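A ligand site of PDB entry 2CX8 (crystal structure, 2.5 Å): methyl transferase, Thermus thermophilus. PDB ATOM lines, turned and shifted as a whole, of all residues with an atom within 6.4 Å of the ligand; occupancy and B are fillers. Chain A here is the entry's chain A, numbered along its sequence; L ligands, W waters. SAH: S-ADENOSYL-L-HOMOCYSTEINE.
O2' of the ligand is in hydrogen-bond range of N of Gly 181 (2.8 Å).
An oxygen (O2') of the ligand is in hydrogen-bond range of the backbone carbonyl oxygen (O) of Ala 158 (2.8 Å).
The backbone NH (N) of Leu 204 lies within hydrogen-bond range of a nitrogen (N1) of the ligand (3.0 Å).
The backbone carbonyl oxygen (O) of Gly 205 is in hydrogen-bond range of a nitrogen (N6) of the ligand, at 3.0 Å.
The backbone NH (N) of His 159 sits close to a nitrogen (N3) of the ligand (3.4 Å).
The backbone NH (N) of Leu 209 sits at hydrogen-bond distance from a nitrogen (N7) of the ligand, at 3.1 Å.
N6 of the ligand sits at hydrogen-bond distance from O of Arg 207 (3.2 Å).
O of Ala 179 lies within hydrogen-bond range of N of Ala 158.
N of Gly 205 sits at hydrogen-bond distance from OG of Ser 203.
The backbone carbonyl oxygen (O) of Val 202 is in hydrogen-bond range of the backbone NH (N) of His 159, at 3.1 Å.
O of Gly 161 is in hydrogen-bond range of ND1 of His 159.
The backbone carbonyl oxygen (O) of Val 157 lies within hydrogen-bond range of the backbone NH (N) of Val 202 (2.9 Å).
Water W1 lies within hydrogen-bond range of N of Phe 186 (3.2 Å) and O3' of the ligand (3.4 Å).
Residues that only touch the ligand: Glu 183, Pro 182, Val 160, Ala 214, Ile 208, Gly 185, Val 180, Val 202, Phe 186, Gly 184, Ala 211 and Ser 203.
Hydrophobic or aromatic side chains within 4 Å of the ligand: Ala 158, Val 160, Val 180, Leu 204, Ile 208, Leu 209, Ala 211 and Ala 214.
Within 4 Å of the ligand: Ala 158, His 159, Val 160, Val 180, Gly 181, Pro 182, Glu 183, Gly 184, Gly 185, Phe 186, Val 202, Ser 203, Leu 204, Gly 205, Arg 207, Ile 208, Leu 209, Ala 211 and Ala 214.
Along chain A the residues within 4 Å of the ligand span positions 158 to 214.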
ATOM      1  N   VAL A 157      29.926 -11.896  11.431  1.00  0.00           N
ATOM      2  CA  VAL A 157      30.472 -10.551  11.287  1.00  0.00           C
ATOM      3  C   VAL A 157      30.289 -10.073   9.869  1.00  0.00           C
ATOM      4  O   VAL A 157      30.703 -10.738   8.916  1.00  0.00           O
ATOM      5  CB  VAL A 157      31.976 -10.452  11.669  1.00  0.00           C
ATOM      6  CG1 VAL A 157      32.816 -11.413  10.828  1.00  0.00           C
ATOM      7  CG2 VAL A 157      32.454  -9.023  11.455  1.00  0.00           C
ATOM      8  N   ALA A 158      29.631  -8.924   9.728  1.00  0.00           N
ATOM      9  CA  ALA A 158      29.404  -8.351   8.415  1.00  0.00           C
ATOM     10  C   ALA A 158      30.738  -7.797   7.896  1.00  0.00           C
ATOM     11  O   ALA A 158      31.323  -6.874   8.472  1.00  0.00           O
ATOM     12  CB  ALA A 158      28.354  -7.239   8.490  1.00  0.00           C
ATOM     13  N   HIS A 159      31.240  -8.373   6.822  1.00  0.00           N
ATOM     14  CA  HIS A 159      32.503  -7.914   6.301  1.00  0.00           C
ATOM     15  C   HIS A 159      32.407  -7.619   4.829  1.00  0.00           C
ATOM     16  O   HIS A 159      31.813  -8.399   4.074  1.00  0.00           O
ATOM     17  CB  HIS A 159      33.594  -8.957   6.546  1.00  0.00           C
ATOM     18  CG  HIS A 159      34.937  -8.565   6.008  1.00  0.00           C
ATOM     19  ND1 HIS A 159      35.852  -9.486   5.554  1.00  0.00           N
ATOM     20  CD2 HIS A 159      35.495  -7.345   5.817  1.00  0.00           C
ATOM     21  CE1 HIS A 159      36.922  -8.857   5.098  1.00  0.00           C
ATOM     22  NE2 HIS A 159      36.732  -7.553   5.251  1.00  0.00           N
ATOM     23  N   VAL A 160      32.969  -6.492   4.407  1.00  0.00           N
ATOM     24  CA  VAL A 160      32.942  -6.126   3.005  1.00  0.00           C
ATOM     25  C   VAL A 160      33.638  -7.225   2.203  1.00  0.00           C
ATOM     26  O   VAL A 160      33.123  -7.686   1.184  1.00  0.00           O
ATOM     27  CB  VAL A 160      33.675  -4.798   2.754  1.00  0.00           C
ATOM     28  CG1 VAL A 160      33.517  -4.398   1.304  1.00  0.00           C
ATOM     29  CG2 VAL A 160      33.119  -3.719   3.672  1.00  0.00           C
ATOM     30  N   GLY A 161      34.806  -7.647   2.679  1.00  0.00           N
ATOM     31  CA  GLY A 161      35.536  -8.693   1.994  1.00  0.00           C
ATOM     32  C   GLY A 161      35.109 -10.087   2.443  1.00  0.00           C
ATOM     33  O   GLY A 161      35.924 -10.862   2.955  1.00  0.00           O
ATOM     34  N   ALA A 162      33.827 -10.393   2.242  1.00  0.00           N
ATOM     35  CA  ALA A 162      33.270 -11.678   2.632  1.00  0.00           C
ATOM     36  C   ALA A 162      32.391 -12.259   1.530  1.00  0.00           C
ATOM     37  O   ALA A 162      31.856 -11.515   0.704  1.00  0.00           O
ATOM     38  CB  ALA A 162      32.478 -11.522   3.920  1.00  0.00           C
ATOM     39  N   ALA A 179      28.401  -8.705  14.509  1.00  0.00           N
ATOM     40  CA  ALA A 179      29.376  -7.634  14.519  1.00  0.00           C
ATOM     41  C   ALA A 179      29.375  -6.817  13.251  1.00  0.00           C
ATOM     42  O   ALA A 179      29.395  -7.356  12.146  1.00  0.00           O
ATOM     43  CB  ALA A 179      30.772  -8.206  14.774  1.00  0.00           C
ATOM     44  N   VAL A 180      29.331  -5.507  13.444  1.00  0.00           N
ATOM     45  CA  VAL A 180      29.340  -4.524  12.355  1.00  0.00           C
ATOM     46  C   VAL A 180      30.444  -3.510  12.651  1.00  0.00           C
ATOM     47  O   VAL A 180      30.658  -3.120  13.807  1.00  0.00           O
ATOM     48  CB  VAL A 180      27.974  -3.789  12.230  1.00  0.00           C
ATOM     49  CG1 VAL A 180      28.058  -2.680  11.186  1.00  0.00           C
ATOM     50  CG2 VAL A 180      26.882  -4.785  11.846  1.00  0.00           C
ATOM     51  N   GLY A 181      31.169  -3.097  11.610  1.00  0.00           N
ATOM     52  CA  GLY A 181      32.233  -2.137  11.798  1.00  0.00           C
ATOM     53  C   GLY A 181      31.748  -0.702  11.685  1.00  0.00           C
ATOM     54  O   GLY A 181      30.618  -0.462  11.268  1.00  0.00           O
ATOM     55  N   PRO A 182      32.607   0.275  12.028  1.00  0.00           N
ATOM     56  CA  PRO A 182      32.296   1.707  11.984  1.00  0.00           C
ATOM     57  C   PRO A 182      32.347   2.187  10.542  1.00  0.00           C
ATOM     58  O   PRO A 182      32.569   1.375   9.643  1.00  0.00           O
ATOM     59  CB  PRO A 182      33.425   2.310  12.820  1.00  0.00           C
ATOM     60  CG  PRO A 182      34.600   1.467  12.408  1.00  0.00           C
ATOM     61  CD  PRO A 182      34.009   0.052  12.425  1.00  0.00           C
ATOM     62  N   GLU A 183      32.183   3.486  10.334  1.00  0.00           N
ATOM     63  CA  GLU A 183      32.203   4.059   8.995  1.00  0.00           C
ATOM     64  C   GLU A 183      33.429   3.604   8.201  1.00  0.00           C
ATOM     65  O   GLU A 183      33.324   3.245   7.038  1.00  0.00           O
ATOM     66  CB  GLU A 183      32.162   5.587   9.040  1.00  0.00           C
ATOM     67  CG  GLU A 183      30.902   6.197   9.664  1.00  0.00           C
ATOM     68  CD  GLU A 183      31.006   6.283  11.175  1.00  0.00           C
ATOM     69  OE1 GLU A 183      31.960   5.684  11.710  1.00  0.00           O
ATOM     70  OE2 GLU A 183      30.141   6.933  11.805  1.00  0.00           O
ATOM     71  N   GLY A 184      34.591   3.630   8.839  1.00  0.00           N
ATOM     72  CA  GLY A 184      35.801   3.222   8.163  1.00  0.00           C
ATOM     73  C   GLY A 184      35.848   1.732   7.896  1.00  0.00           C
ATOM     74  O   GLY A 184      36.520   1.269   6.979  1.00  0.00           O
ATOM     75  N   GLY A 185      35.130   0.965   8.717  1.00  0.00           N
ATOM     76  CA  GLY A 185      35.088  -0.480   8.568  1.00  0.00           C
ATOM     77  C   GLY A 185      36.102  -1.209   9.430  1.00  0.00           C
ATOM     78  O   GLY A 185      37.001  -0.583   9.991  1.00  0.00           O
ATOM     79  N   PHE A 186      35.953  -2.519   9.556  1.00  0.00           N
ATOM     80  CA  PHE A 186      36.909  -3.315  10.331  1.00  0.00           C
ATOM     81  C   PHE A 186      38.222  -3.432   9.550  1.00  0.00           C
ATOM     82  O   PHE A 186      38.225  -3.540   8.316  1.00  0.00           O
ATOM     83  CB  PHE A 186      36.382  -4.728  10.588  1.00  0.00           C
ATOM     84  CG  PHE A 186      35.315  -4.808  11.629  1.00  0.00           C
ATOM     85  CD1 PHE A 186      34.083  -5.374  11.325  1.00  0.00           C
ATOM     86  CD2 PHE A 186      35.530  -4.309  12.900  1.00  0.00           C
ATOM     87  CE1 PHE A 186      33.072  -5.464  12.293  1.00  0.00           C
ATOM     88  CE2 PHE A 186      34.537  -4.393  13.881  1.00  0.00           C
ATOM     89  CZ  PHE A 186      33.294  -4.977  13.568  1.00  0.00           C
ATOM     90  N   VAL A 202      30.435 -12.589   6.757  1.00  0.00           N
ATOM     91  CA  VAL A 202      29.291 -12.732   5.894  1.00  0.00           C
ATOM     92  C   VAL A 202      29.095 -11.515   5.005  1.00  0.00           C
ATOM     93  O   VAL A 202      29.411 -10.395   5.378  1.00  0.00           O
ATOM     94  CB  VAL A 202      27.987 -13.021   6.694  1.00  0.00           C
ATOM     95  CG1 VAL A 202      28.142 -14.334   7.478  1.00  0.00           C
ATOM     96  CG2 VAL A 202      27.657 -11.857   7.633  1.00  0.00           C
ATOM     97  N   SER A 203      28.571 -11.773   3.816  1.00  0.00           N
ATOM     98  CA  SER A 203      28.294 -10.734   2.833  1.00  0.00           C
ATOM     99  C   SER A 203      26.898 -10.179   3.026  1.00  0.00           C
ATOM    100  O   SER A 203      25.967 -10.904   3.343  1.00  0.00           O
ATOM    101  CB  SER A 203      28.373 -11.316   1.433  1.00  0.00           C
ATOM    102  OG  SER A 203      27.636 -10.513   0.527  1.00  0.00           O
ATOM    103  N   LEU A 204      26.752  -8.879   2.807  1.00  0.00           N
ATOM    104  CA  LEU A 204      25.446  -8.247   2.889  1.00  0.00           C
ATOM    105  C   LEU A 204      25.162  -7.723   1.494  1.00  0.00           C
ATOM    106  O   LEU A 204      24.429  -6.754   1.324  1.00  0.00           O
ATOM    107  CB  LEU A 204      25.455  -7.093   3.900  1.00  0.00           C
ATOM    108  CG  LEU A 204      25.405  -7.516   5.363  1.00  0.00           C
ATOM    109  CD1 LEU A 204      25.352  -6.278   6.258  1.00  0.00           C
ATOM    110  CD2 LEU A 204      24.174  -8.388   5.599  1.00  0.00           C
ATOM    111  N   GLY A 205      25.772  -8.370   0.507  1.00  0.00           N
ATOM    112  CA  GLY A 205      25.572  -7.960  -0.872  1.00  0.00           C
ATOM    113  C   GLY A 205      26.745  -7.215  -1.484  1.00  0.00           C
ATOM    114  O   GLY A 205      27.758  -6.961  -0.828  1.00  0.00           O
ATOM    115  N   ARG A 206      26.583  -6.836  -2.745  1.00  0.00           N
ATOM    116  CA  ARG A 206      27.625  -6.155  -3.517  1.00  0.00           C
ATOM    117  C   ARG A 206      27.807  -4.656  -3.300  1.00  0.00           C
ATOM    118  O   ARG A 206      28.816  -4.103  -3.712  1.00  0.00           O
ATOM    119  CB  ARG A 206      27.381  -6.419  -4.992  1.00  0.00           C
ATOM    120  CG  ARG A 206      26.965  -7.848  -5.272  1.00  0.00           C
ATOM    121  CD  ARG A 206      26.596  -8.083  -6.731  1.00  0.00           C
ATOM    122  NE  ARG A 206      25.709  -9.233  -6.888  1.00  0.00           N
ATOM    123  CZ  ARG A 206      25.383  -9.796  -8.049  1.00  0.00           C
ATOM    124  NH1 ARG A 206      25.888  -9.338  -9.185  1.00  0.00           N
ATOM    125  NH2 ARG A 206      24.546 -10.827  -8.069  1.00  0.00           N
ATOM    126  N   ARG A 207      26.851  -3.990  -2.656  1.00  0.00           N
ATOM    127  CA  ARG A 207      26.985  -2.548  -2.444  1.00  0.00           C
ATOM    128  C   ARG A 207      27.478  -2.210  -1.044  1.00  0.00           C
ATOM    129  O   ARG A 207      27.132  -2.900  -0.092  1.00  0.00           O
ATOM    130  CB  ARG A 207      25.642  -1.871  -2.684  1.00  0.00           C
ATOM    131  CG  ARG A 207      25.103  -2.079  -4.095  1.00  0.00           C
ATOM    132  CD  ARG A 207      23.600  -2.120  -4.041  1.00  0.00           C
ATOM    133  NE  ARG A 207      23.173  -3.187  -3.164  1.00  0.00           N
ATOM    134  CZ  ARG A 207      23.122  -4.476  -3.504  1.00  0.00           C
ATOM    135  NH1 ARG A 207      23.482  -4.861  -4.719  1.00  0.00           N
ATOM    136  NH2 ARG A 207      22.727  -5.383  -2.617  1.00  0.00           N
ATOM    137  N   ILE A 208      28.312  -1.176  -0.941  1.00  0.00           N
ATOM    138  CA  ILE A 208      28.800  -0.769   0.381  1.00  0.00           C
ATOM    139  C   ILE A 208      27.602  -0.165   1.094  1.00  0.00           C
ATOM    140  O   ILE A 208      26.878   0.644   0.528  1.00  0.00           O
ATOM    141  CB  ILE A 208      29.923   0.292   0.270  1.00  0.00           C
ATOM    142  CG1 ILE A 208      31.211  -0.355  -0.242  1.00  0.00           C
ATOM    143  CG2 ILE A 208      30.143   0.946   1.630  1.00  0.00           C
ATOM    144  CD1 ILE A 208      32.291   0.652  -0.646  1.00  0.00           C
ATOM    145  N   LEU A 209      27.378  -0.578   2.319  1.00  0.00           N
ATOM    146  CA  LEU A 209      26.237  -0.078   3.056  1.00  0.00           C
ATOM    147  C   LEU A 209      26.685   0.722   4.251  1.00  0.00           C
ATOM    148  O   LEU A 209      27.790   0.497   4.751  1.00  0.00           O
ATOM    149  CB  LEU A 209      25.384  -1.253   3.552  1.00  0.00           C
ATOM    150  CG  LEU A 209      24.994  -2.336   2.537  1.00  0.00           C
ATOM    151  CD1 LEU A 209      24.362  -3.499   3.296  1.00  0.00           C
ATOM    152  CD2 LEU A 209      24.042  -1.762   1.462  1.00  0.00           C
ATOM    153  N   ARG A 210      25.851   1.653   4.714  1.00  0.00           N
ATOM    154  CA  ARG A 210      26.202   2.402   5.908  1.00  0.00           C
ATOM    155  C   ARG A 210      26.156   1.407   7.068  1.00  0.00           C
ATOM    156  O   ARG A 210      25.374   0.453   7.049  1.00  0.00           O
ATOM    157  CB  ARG A 210      25.175   3.515   6.193  1.00  0.00           C
ATOM    158  CG  ARG A 210      25.252   4.736   5.297  1.00  0.00           C
ATOM    159  CD  ARG A 210      24.107   5.701   5.613  1.00  0.00           C
ATOM    160  NE  ARG A 210      22.822   5.178   5.182  1.00  0.00           N
ATOM    161  CZ  ARG A 210      21.636   5.706   5.490  1.00  0.00           C
ATOM    162  NH1 ARG A 210      21.566   6.793   6.241  1.00  0.00           N
ATOM    163  NH2 ARG A 210      20.523   5.153   5.026  1.00  0.00           N
ATOM    164  N   ALA A 211      26.988   1.621   8.083  1.00  0.00           N
ATOM    165  CA  ALA A 211      27.010   0.763   9.248  1.00  0.00           C
ATOM    166  C   ALA A 211      25.608   0.551   9.834  1.00  0.00           C
ATOM    167  O   ALA A 211      25.275  -0.549  10.306  1.00  0.00           O
ATOM    168  CB  ALA A 211      27.927   1.367  10.319  1.00  0.00           C
ATOM    169  N   GLU A 212      24.784   1.617   9.824  1.00  0.00           N
ATOM    170  CA  GLU A 212      23.421   1.549  10.347  1.00  0.00           C
ATOM    171  C   GLU A 212      22.576   0.546   9.558  1.00  0.00           C
ATOM    172  O   GLU A 212      21.886  -0.290  10.120  1.00  0.00           O
ATOM    173  CB  GLU A 212      22.722   2.920  10.298  1.00  0.00           C
ATOM    174  CG  GLU A 212      23.426   4.030  11.044  1.00  0.00           C
ATOM    175  CD  GLU A 212      24.235   4.929  10.097  1.00  0.00           C
ATOM    176  OE1 GLU A 212      25.278   4.452   9.577  1.00  0.00           O
ATOM    177  OE2 GLU A 212      23.799   6.083   9.877  1.00  0.00           O
ATOM    178  N   ALA A 214      23.726  -1.815   7.643  1.00  0.00           N
ATOM    179  CA  ALA A 214      24.354  -3.121   7.715  1.00  0.00           C
ATOM    180  C   ALA A 214      23.827  -3.861   8.927  1.00  0.00           C
ATOM    181  O   ALA A 214      23.439  -5.016   8.841  1.00  0.00           O
ATOM    182  CB  ALA A 214      25.878  -2.993   7.774  1.00  0.00           C
ATOM    183  N   ALA A 215      23.832  -3.191  10.081  1.00  0.00           N
ATOM    184  CA  ALA A 215      23.319  -3.819  11.295  1.00  0.00           C
ATOM    185  C   ALA A 215      21.843  -4.164  11.078  1.00  0.00           C
ATOM    186  O   ALA A 215      21.383  -5.240  11.455  1.00  0.00           O
ATOM    187  CB  ALA A 215      23.490  -2.870  12.507  1.00  0.00           C
HETATM  188  N   SAH L   1      34.556  -1.167   5.002  1.00  0.00           N
HETATM  189  CA  SAH L   1      33.777  -0.258   4.145  1.00  0.00           C
HETATM  190  CB  SAH L   1      33.393   0.996   4.939  1.00  0.00           C
HETATM  191  CG  SAH L   1      32.629   0.657   6.221  1.00  0.00           C
HETATM  192  SD  SAH L   1      30.922   0.044   5.976  1.00  0.00           S
HETATM  193  C   SAH L   1      34.636   0.155   2.952  1.00  0.00           C
HETATM  194  O   SAH L   1      35.598   0.920   3.186  1.00  0.00           O
HETATM  195  OXT SAH L   1      34.319  -0.305   1.836  1.00  0.00           O
HETATM  196  C5' SAH L   1      30.478  -0.138   7.744  1.00  0.00           C
HETATM  197  C4' SAH L   1      30.207  -1.582   8.158  1.00  0.00           C
HETATM  198  O4' SAH L   1      29.001  -2.079   7.578  1.00  0.00           O
HETATM  199  C3' SAH L   1      31.316  -2.531   7.697  1.00  0.00           C
HETATM  200  O3' SAH L   1      32.377  -2.502   8.645  1.00  0.00           O
HETATM  201  C2' SAH L   1      30.567  -3.857   7.803  1.00  0.00           C
HETATM  202  O2' SAH L   1      30.461  -4.263   9.170  1.00  0.00           O
HETATM  203  C1' SAH L   1      29.183  -3.472   7.271  1.00  0.00           C
HETATM  204  N9  SAH L   1      29.034  -3.615   5.807  1.00  0.00           N
HETATM  205  C8  SAH L   1      28.774  -2.625   4.949  1.00  0.00           C
HETATM  206  N7  SAH L   1      28.557  -3.126   3.737  1.00  0.00           N
HETATM  207  C5  SAH L   1      28.701  -4.446   3.819  1.00  0.00           C
HETATM  208  C6  SAH L   1      28.583  -5.501   2.920  1.00  0.00           C
HETATM  209  N6  SAH L   1      28.270  -5.277   1.643  1.00  0.00           N
HETATM  210  N1  SAH L   1      28.774  -6.759   3.348  1.00  0.00           N
HETATM  211  C2  SAH L   1      29.070  -7.010   4.621  1.00  0.00           C
HETATM  212  N3  SAH L   1      29.179  -6.043   5.501  1.00  0.00           N
HETATM  213  C4  SAH L   1      29.002  -4.760   5.135  1.00  0.00           C
HETATM  214  O   HOH W   1      34.876  -4.185   7.082  1.00  0.00           O
